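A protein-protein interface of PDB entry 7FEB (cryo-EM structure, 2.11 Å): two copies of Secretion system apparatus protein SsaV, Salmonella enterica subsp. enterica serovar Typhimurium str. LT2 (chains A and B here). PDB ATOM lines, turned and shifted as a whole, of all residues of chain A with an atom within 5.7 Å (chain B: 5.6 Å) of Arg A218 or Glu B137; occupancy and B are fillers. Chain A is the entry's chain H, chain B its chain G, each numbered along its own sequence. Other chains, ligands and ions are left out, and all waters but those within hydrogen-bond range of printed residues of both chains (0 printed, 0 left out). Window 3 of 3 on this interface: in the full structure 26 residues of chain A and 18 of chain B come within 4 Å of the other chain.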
ATOM      1  N   ARG A 189     -12.484  16.165  15.605  1.00  0.00           N
ATOM      2  CA  ARG A 189     -13.348  17.223  16.197  1.00  0.00           C
ATOM      3  C   ARG A 189     -12.603  18.562  16.189  1.00  0.00           C
ATOM      4  O   ARG A 189     -13.206  19.571  15.769  1.00  0.00           O
ATOM      5  CB  ARG A 189     -13.767  16.836  17.618  1.00  0.00           C
ATOM      6  CG  ARG A 189     -15.069  17.474  18.078  1.00  0.00           C
ATOM      7  CD  ARG A 189     -15.099  17.713  19.576  1.00  0.00           C
ATOM      8  NE  ARG A 189     -14.107  18.689  20.003  1.00  0.00           N
ATOM      9  CZ  ARG A 189     -14.365  19.732  20.785  1.00  0.00           C
ATOM     10  NH1 ARG A 189     -15.592  19.937  21.231  1.00  0.00           N
ATOM     11  NH2 ARG A 189     -13.396  20.565  21.118  1.00  0.00           N
ATOM     12  N   ILE A 214      -1.033  24.529  13.796  1.00  0.00           N
ATOM     13  CA  ILE A 214      -0.896  25.379  14.977  1.00  0.00           C
ATOM     14  C   ILE A 214      -1.861  24.931  16.067  1.00  0.00           C
ATOM     15  O   ILE A 214      -1.495  24.846  17.245  1.00  0.00           O
ATOM     16  CB  ILE A 214      -1.106  26.857  14.600  1.00  0.00           C
ATOM     17  CG1 ILE A 214       0.105  27.387  13.831  1.00  0.00           C
ATOM     18  CG2 ILE A 214      -1.353  27.698  15.841  1.00  0.00           C
ATOM     19  CD1 ILE A 214      -0.235  28.465  12.829  1.00  0.00           C
ATOM     20  N   ALA A 215      -3.106  24.624  15.692  1.00  0.00           N
ATOM     21  CA  ALA A 215      -4.084  24.170  16.675  1.00  0.00           C
ATOM     22  C   ALA A 215      -3.712  22.819  17.275  1.00  0.00           C
ATOM     23  O   ALA A 215      -4.123  22.510  18.398  1.00  0.00           O
ATOM     24  CB  ALA A 215      -5.473  24.101  16.042  1.00  0.00           C
ATOM     25  N   LEU A 216      -2.941  22.005  16.553  1.00  0.00           N
ATOM     26  CA  LEU A 216      -2.564  20.671  17.003  1.00  0.00           C
ATOM     27  C   LEU A 216      -1.151  20.619  17.571  1.00  0.00           C
ATOM     28  O   LEU A 216      -0.585  19.528  17.696  1.00  0.00           O
ATOM     29  CB  LEU A 216      -2.696  19.670  15.855  1.00  0.00           C
ATOM     30  CG  LEU A 216      -4.078  19.111  15.526  1.00  0.00           C
ATOM     31  CD1 LEU A 216      -4.039  18.395  14.188  1.00  0.00           C
ATOM     32  CD2 LEU A 216      -4.556  18.177  16.620  1.00  0.00           C
ATOM     33  N   ARG A 217      -0.573  21.769  17.923  1.00  0.00           N
ATOM     34  CA  ARG A 217       0.837  21.808  18.300  1.00  0.00           C
ATOM     35  C   ARG A 217       1.124  20.980  19.547  1.00  0.00           C
ATOM     36  O   ARG A 217       2.224  20.430  19.681  1.00  0.00           O
ATOM     37  CB  ARG A 217       1.290  23.255  18.499  1.00  0.00           C
ATOM     38  CG  ARG A 217       0.735  23.935  19.736  1.00  0.00           C
ATOM     39  CD  ARG A 217       0.801  25.453  19.603  1.00  0.00           C
ATOM     40  NE  ARG A 217       0.722  26.169  20.875  1.00  0.00           N
ATOM     41  CZ  ARG A 217       1.484  25.946  21.940  1.00  0.00           C
ATOM     42  NH1 ARG A 217       2.482  25.078  21.916  1.00  0.00           N
ATOM     43  NH2 ARG A 217       1.252  26.634  23.055  1.00  0.00           N
ATOM     44  N   ARG A 218       0.118  20.839  20.420  1.00  0.00           N
ATOM     45  CA  ARG A 218       0.268  20.073  21.686  1.00  0.00           C
ATOM     46  C   ARG A 218       0.556  18.610  21.340  1.00  0.00           C
ATOM     47  O   ARG A 218       1.504  18.038  21.912  1.00  0.00           O
ATOM     48  CB  ARG A 218      -0.996  20.198  22.541  1.00  0.00           C
ATOM     49  CG  ARG A 218      -1.049  19.234  23.717  1.00  0.00           C
ATOM     50  CD  ARG A 218      -2.105  19.623  24.735  1.00  0.00           C
ATOM     51  NE  ARG A 218      -3.448  19.263  24.301  1.00  0.00           N
ATOM     52  CZ  ARG A 218      -4.525  20.019  24.480  1.00  0.00           C
ATOM     53  NH1 ARG A 218      -4.420  21.187  25.089  1.00  0.00           N
ATOM     54  NH2 ARG A 218      -5.703  19.605  24.051  1.00  0.00           N
ATOM     55  N   HIS A 219      -0.243  18.042  20.434  1.00  0.00           N
ATOM     56  CA  HIS A 219      -0.061  16.660  20.006  1.00  0.00           C
ATOM     57  C   HIS A 219       1.225  16.493  19.208  1.00  0.00           C
ATOM     58  O   HIS A 219       1.907  15.471  19.326  1.00  0.00           O
ATOM     59  CB  HIS A 219      -1.256  16.190  19.180  1.00  0.00           C
ATOM     60  CG  HIS A 219      -0.957  14.998  18.327  1.00  0.00           C
ATOM     61  ND1 HIS A 219      -0.434  15.104  17.056  1.00  0.00           N
ATOM     62  CD2 HIS A 219      -1.082  13.672  18.572  1.00  0.00           C
ATOM     63  CE1 HIS A 219      -0.256  13.896  16.553  1.00  0.00           C
ATOM     64  NE2 HIS A 219      -0.646  13.010  17.452  1.00  0.00           N
ATOM     65  N   ILE A 220       1.558  17.478  18.372  1.00  0.00           N
ATOM     66  CA  ILE A 220       2.768  17.391  17.560  1.00  0.00           C
ATOM     67  C   ILE A 220       4.002  17.312  18.452  1.00  0.00           C
ATOM     68  O   ILE A 220       4.888  16.475  18.244  1.00  0.00           O
ATOM     69  CB  ILE A 220       2.846  18.581  16.587  1.00  0.00           C
ATOM     70  CG1 ILE A 220       1.744  18.476  15.532  1.00  0.00           C
ATOM     71  CG2 ILE A 220       4.213  18.645  15.927  1.00  0.00           C
ATOM     72  CD1 ILE A 220       1.707  19.639  14.571  1.00  0.00           C
ATOM     73  N   LEU A 221       4.069  18.174  19.470  1.00  0.00           N
ATOM     74  CA  LEU A 221       5.208  18.138  20.383  1.00  0.00           C
ATOM     75  C   LEU A 221       5.206  16.870  21.230  1.00  0.00           C
ATOM     76  O   LEU A 221       6.272  16.320  21.525  1.00  0.00           O
ATOM     77  CB  LEU A 221       5.217  19.380  21.273  1.00  0.00           C
ATOM     78  CG  LEU A 221       5.241  20.730  20.553  1.00  0.00           C
ATOM     79  CD1 LEU A 221       5.544  21.852  21.531  1.00  0.00           C
ATOM     80  CD2 LEU A 221       6.254  20.716  19.420  1.00  0.00           C
ATOM     81  N   ARG A 222       4.008  16.395  21.583  1.00  0.00           N
ATOM     82  CA  ARG A 222       3.865  15.160  22.400  1.00  0.00           C
ATOM     83  C   ARG A 222       4.401  13.962  21.605  1.00  0.00           C
ATOM     84  O   ARG A 222       5.057  13.095  22.216  1.00  0.00           O
ATOM     85  CB  ARG A 222       2.401  14.948  22.798  1.00  0.00           C
ATOM     86  CG  ARG A 222       2.216  14.298  24.161  1.00  0.00           C
ATOM     87  CD  ARG A 222       1.993  12.800  24.059  1.00  0.00           C
ATOM     88  NE  ARG A 222       0.922  12.464  23.132  1.00  0.00           N
ATOM     89  CZ  ARG A 222       0.522  11.227  22.863  1.00  0.00           C
ATOM     90  NH1 ARG A 222       1.107  10.198  23.450  1.00  0.00           N
ATOM     91  NH2 ARG A 222      -0.461  11.023  22.004  1.00  0.00           N
ATOM     92  N   ARG A 223       4.130  13.924  20.296  1.00  0.00           N
ATOM     93  CA  ARG A 223       4.584  12.835  19.439  1.00  0.00           C
ATOM     94  C   ARG A 223       6.072  12.951  19.138  1.00  0.00           C
ATOM     95  O   ARG A 223       6.787  11.942  19.130  1.00  0.00           O
ATOM     96  CB  ARG A 223       3.773  12.819  18.144  1.00  0.00           C
ATOM     97  CG  ARG A 223       3.663  11.451  17.492  1.00  0.00           C
ATOM     98  CD  ARG A 223       2.746  10.535  18.285  1.00  0.00           C
ATOM     99  NE  ARG A 223       1.413  10.449  17.699  1.00  0.00           N
ATOM    100  CZ  ARG A 223       0.364   9.913  18.307  1.00  0.00           C
ATOM    101  NH1 ARG A 223       0.456   9.404  19.524  1.00  0.00           N
ATOM    102  NH2 ARG A 223      -0.808   9.892  17.680  1.00  0.00           N
ATOM    103  N   GLU A 311       4.550  26.860  16.485  1.00  0.00           N
ATOM    104  CA  GLU A 311       4.202  25.496  16.860  1.00  0.00           C
ATOM    105  C   GLU A 311       4.841  25.059  18.172  1.00  0.00           C
ATOM    106  O   GLU A 311       4.395  24.068  18.760  1.00  0.00           O
ATOM    107  CB  GLU A 311       4.595  24.525  15.745  1.00  0.00           C
ATOM    108  CG  GLU A 311       3.490  24.284  14.729  1.00  0.00           C
ATOM    109  CD  GLU A 311       4.021  23.944  13.352  1.00  0.00           C
ATOM    110  OE1 GLU A 311       5.009  23.184  13.266  1.00  0.00           O
ATOM    111  OE2 GLU A 311       3.451  24.435  12.357  1.00  0.00           O
ATOM    112  N   LEU B  59      -7.340  14.305  27.335  1.00  0.00           N
ATOM    113  CA  LEU B  59      -8.423  14.976  26.631  1.00  0.00           C
ATOM    114  C   LEU B  59      -8.316  14.638  25.151  1.00  0.00           C
ATOM    115  O   LEU B  59      -7.320  14.980  24.507  1.00  0.00           O
ATOM    116  CB  LEU B  59      -8.365  16.490  26.830  1.00  0.00           C
ATOM    117  CG  LEU B  59      -8.152  17.028  28.242  1.00  0.00           C
ATOM    118  CD1 LEU B  59      -7.877  18.515  28.189  1.00  0.00           C
ATOM    119  CD2 LEU B  59      -9.345  16.741  29.116  1.00  0.00           C
ATOM    120  N   TYR B  60      -9.346  13.982  24.620  1.00  0.00           N
ATOM    121  CA  TYR B  60      -9.352  13.530  23.230  1.00  0.00           C
ATOM    122  C   TYR B  60      -8.104  12.704  22.926  1.00  0.00           C
ATOM    123  O   TYR B  60      -7.438  12.888  21.906  1.00  0.00           O
ATOM    124  CB  TYR B  60      -9.507  14.712  22.271  1.00  0.00           C
ATOM    125  CG  TYR B  60     -10.788  15.475  22.515  1.00  0.00           C
ATOM    126  CD1 TYR B  60     -12.007  14.977  22.082  1.00  0.00           C
ATOM    127  CD2 TYR B  60     -10.784  16.676  23.212  1.00  0.00           C
ATOM    128  CE1 TYR B  60     -13.182  15.661  22.319  1.00  0.00           C
ATOM    129  CE2 TYR B  60     -11.953  17.366  23.452  1.00  0.00           C
ATOM    130  CZ  TYR B  60     -13.148  16.854  23.003  1.00  0.00           C
ATOM    131  OH  TYR B  60     -14.317  17.539  23.238  1.00  0.00           O
ATOM    132  N   GLU B  62      -5.192  12.702  24.125  1.00  0.00           N
ATOM    133  CA  GLU B  62      -3.894  13.343  24.269  1.00  0.00           C
ATOM    134  C   GLU B  62      -3.598  13.535  25.745  1.00  0.00           C
ATOM    135  O   GLU B  62      -4.364  14.227  26.433  1.00  0.00           O
ATOM    136  CB  GLU B  62      -3.859  14.684  23.540  1.00  0.00           C
ATOM    137  CG  GLU B  62      -3.768  14.573  22.029  1.00  0.00           C
ATOM    138  CD  GLU B  62      -2.540  13.811  21.572  1.00  0.00           C
ATOM    139  OE1 GLU B  62      -1.415  14.310  21.785  1.00  0.00           O
ATOM    140  OE2 GLU B  62      -2.699  12.712  21.001  1.00  0.00           O
ATOM    141  N   PRO B  63      -2.525  12.952  26.282  1.00  0.00           N
ATOM    142  CA  PRO B  63      -2.255  13.095  27.719  1.00  0.00           C
ATOM    143  C   PRO B  63      -1.968  14.533  28.113  1.00  0.00           C
ATOM    144  O   PRO B  63      -0.943  15.102  27.725  1.00  0.00           O
ATOM    145  CB  PRO B  63      -1.031  12.198  27.938  1.00  0.00           C
ATOM    146  CG  PRO B  63      -0.387  12.102  26.597  1.00  0.00           C
ATOM    147  CD  PRO B  63      -1.500  12.147  25.599  1.00  0.00           C
ATOM    148  N   VAL B  64      -2.872  15.131  28.886  1.00  0.00           N
ATOM    149  CA  VAL B  64      -2.686  16.503  29.342  1.00  0.00           C
ATOM    150  C   VAL B  64      -2.263  16.578  30.803  1.00  0.00           C
ATOM    151  O   VAL B  64      -1.697  17.602  31.215  1.00  0.00           O
ATOM    152  CB  VAL B  64      -3.959  17.345  29.119  1.00  0.00           C
ATOM    153  CG1 VAL B  64      -4.413  17.256  27.672  1.00  0.00           C
ATOM    154  CG2 VAL B  64      -5.063  16.905  30.065  1.00  0.00           C
ATOM    155  N   HIS B 134      -8.992  23.391  31.095  1.00  0.00           N
ATOM    156  CA  HIS B 134      -9.280  23.121  29.693  1.00  0.00           C
ATOM    157  C   HIS B 134     -10.778  23.121  29.418  1.00  0.00           C
ATOM    158  O   HIS B 134     -11.281  22.323  28.627  1.00  0.00           O
ATOM    159  CB  HIS B 134      -8.662  21.793  29.266  1.00  0.00           C
ATOM    160  CG  HIS B 134      -7.205  21.676  29.581  1.00  0.00           C
ATOM    161  ND1 HIS B 134      -6.232  22.328  28.856  1.00  0.00           N
ATOM    162  CD2 HIS B 134      -6.555  20.984  30.546  1.00  0.00           C
ATOM    163  CE1 HIS B 134      -5.045  22.043  29.360  1.00  0.00           C
ATOM    164  NE2 HIS B 134      -5.213  21.228  30.386  1.00  0.00           N
ATOM    165  N   MET B 135     -11.514  24.021  30.076  1.00  0.00           N
ATOM    166  CA  MET B 135     -12.956  24.092  29.861  1.00  0.00           C
ATOM    167  C   MET B 135     -13.282  24.503  28.432  1.00  0.00           C
ATOM    168  O   MET B 135     -14.205  23.957  27.815  1.00  0.00           O
ATOM    169  CB  MET B 135     -13.587  25.062  30.858  1.00  0.00           C
ATOM    170  CG  MET B 135     -14.161  24.383  32.082  1.00  0.00           C
ATOM    171  SD  MET B 135     -15.462  23.214  31.663  1.00  0.00           S
ATOM    172  CE  MET B 135     -15.740  22.449  33.253  1.00  0.00           C
ATOM    173  N   GLY B 136     -12.518  25.445  27.878  1.00  0.00           N
ATOM    174  CA  GLY B 136     -12.752  25.923  26.527  1.00  0.00           C
ATOM    175  C   GLY B 136     -12.595  24.865  25.456  1.00  0.00           C
ATOM    176  O   GLY B 136     -13.035  25.086  24.322  1.00  0.00           O
ATOM    177  N   GLU B 137     -11.984  23.731  25.780  1.00  0.00           N
ATOM    178  CA  GLU B 137     -11.857  22.628  24.841  1.00  0.00           C
ATOM    179  C   GLU B 137     -13.096  21.748  24.795  1.00  0.00           C
ATOM    180  O   GLU B 137     -13.114  20.772  24.040  1.00  0.00           O
ATOM    181  CB  GLU B 137     -10.632  21.779  25.190  1.00  0.00           C
ATOM    182  CG  GLU B 137      -9.318  22.535  25.104  1.00  0.00           C
ATOM    183  CD  GLU B 137      -8.115  21.655  25.377  1.00  0.00           C
ATOM    184  OE1 GLU B 137      -8.152  20.463  25.008  1.00  0.00           O
ATOM    185  OE2 GLU B 137      -7.131  22.157  25.960  1.00  0.00           O
ATOM    186  N   PHE B 138     -14.128  22.060  25.578  1.00  0.00           N
ATOM    187  CA  PHE B 138     -15.352  21.272  25.585  1.00  0.00           C
ATOM    188  C   PHE B 138     -16.555  22.041  25.056  1.00  0.00           C
ATOM    189  O   PHE B 138     -17.684  21.561  25.182  1.00  0.00           O
ATOM    190  CB  PHE B 138     -15.633  20.752  26.994  1.00  0.00           C
ATOM    191  CG  PHE B 138     -14.585  19.813  27.505  1.00  0.00           C
ATOM    192  CD1 PHE B 138     -14.517  18.515  27.034  1.00  0.00           C
ATOM    193  CD2 PHE B 138     -13.661  20.231  28.444  1.00  0.00           C
ATOM    194  CE1 PHE B 138     -13.549  17.649  27.495  1.00  0.00           C
ATOM    195  CE2 PHE B 138     -12.692  19.369  28.909  1.00  0.00           C
ATOM    196  CZ  PHE B 138     -12.638  18.076  28.433  1.00  0.00           C
ATOM    197  N   ILE B 139     -16.347  23.215  24.470  1.00  0.00           N
ATOM    198  CA  ILE B 139     -17.431  24.018  23.917  1.00  0.00           C
ATOM    199  C   ILE B 139     -17.085  24.357  22.469  1.00  0.00           C
ATOM    200  O   ILE B 139     -16.226  25.207  22.210  1.00  0.00           O
ATOM    201  CB  ILE B 139     -17.703  25.287  24.747  1.00  0.00           C
ATOM    202  CG1 ILE B 139     -18.939  26.022  24.221  1.00  0.00           C
ATOM    203  CG2 ILE B 139     -16.472  26.187  24.831  1.00  0.00           C
ATOM    204  CD1 ILE B 139     -19.450  27.090  25.157  1.00  0.00           C
ATOM    205  N   GLN B 176     -17.321  29.955  23.272  1.00  0.00           N
ATOM    206  CA  GLN B 176     -15.979  29.485  23.591  1.00  0.00           C
ATOM    207  C   GLN B 176     -15.123  30.606  24.160  1.00  0.00           C
ATOM    208  O   GLN B 176     -14.364  30.394  25.111  1.00  0.00           O
ATOM    209  CB  GLN B 176     -15.330  28.887  22.342  1.00  0.00           C
ATOM    210  CG  GLN B 176     -14.203  27.910  22.630  1.00  0.00           C
ATOM    211  CD  GLN B 176     -12.879  28.602  22.875  1.00  0.00           C
ATOM    212  OE1 GLN B 176     -12.629  29.691  22.359  1.00  0.00           O
ATOM    213  NE2 GLN B 176     -12.022  27.974  23.669  1.00  0.00           N
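The side-chain hydroxyl (OH) of Tyr B60 sits close to the guanidinium group (NH1) of Arg A189 (3.4 Å).
The side-chain carboxylate (OE2) of Glu B62 lies within salt-bridge range of the guanidinium group (NH2) of Arg A222, 3.0 Å away.
The backbone carbonyl oxygen (O) of Glu B137 lies within hydrogen-bond range of the guanidinium group (NH2) of Arg A189 (2.9 Å).
OE1 of Glu B137 is in salt-bridge range of NH2 of Arg A218 (2.8 Å).
A ring nitrogen (ND1) of His B134 sits at hydrogen-bond distance from the side-chain carboxylate (OE2) of Glu B137.
NH2 of Arg A223 is in hydrogen-bond range of NE2 of His A219, 3.1 Å away.
Among the printed residues, pairs that only touch across the chains: His A219 with Glu B62 and Arg A222 with Pro B63.
Of the printed residues of chain B, Arg A189 touches Tyr B60 (3.3 Å) and Glu B137 (2.9 Å).
Printed residues of chain A within 4 Å of Tyr B60: Arg A189.
Of the printed residues of chain A, Glu B62 touches His A219 and Arg A222.
Printed residues of chain A within 4 Å of Pro B63: Arg A222.
The nearest residue of chain B that does not touch Arg A218 is Val B64 (4.04 Å).
The nearest printed residue of chain A that does not touch Glu B137 is Ala A215 (8.0 Å).
The nearest printed residue of chain A that does not touch Tyr B60 is Arg A218 (5.9 Å).
Hydrophobic or aromatic side chains of chain B that line the printed part of chain A: Tyr B60 and Pro B63.
Among the printed residues, 6 pairs touch across the chains.
No position is printed for both chains.
Of the 6 pairs that touch across the chains among the printed residues, none has its exchanged pair printed and touching as well.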
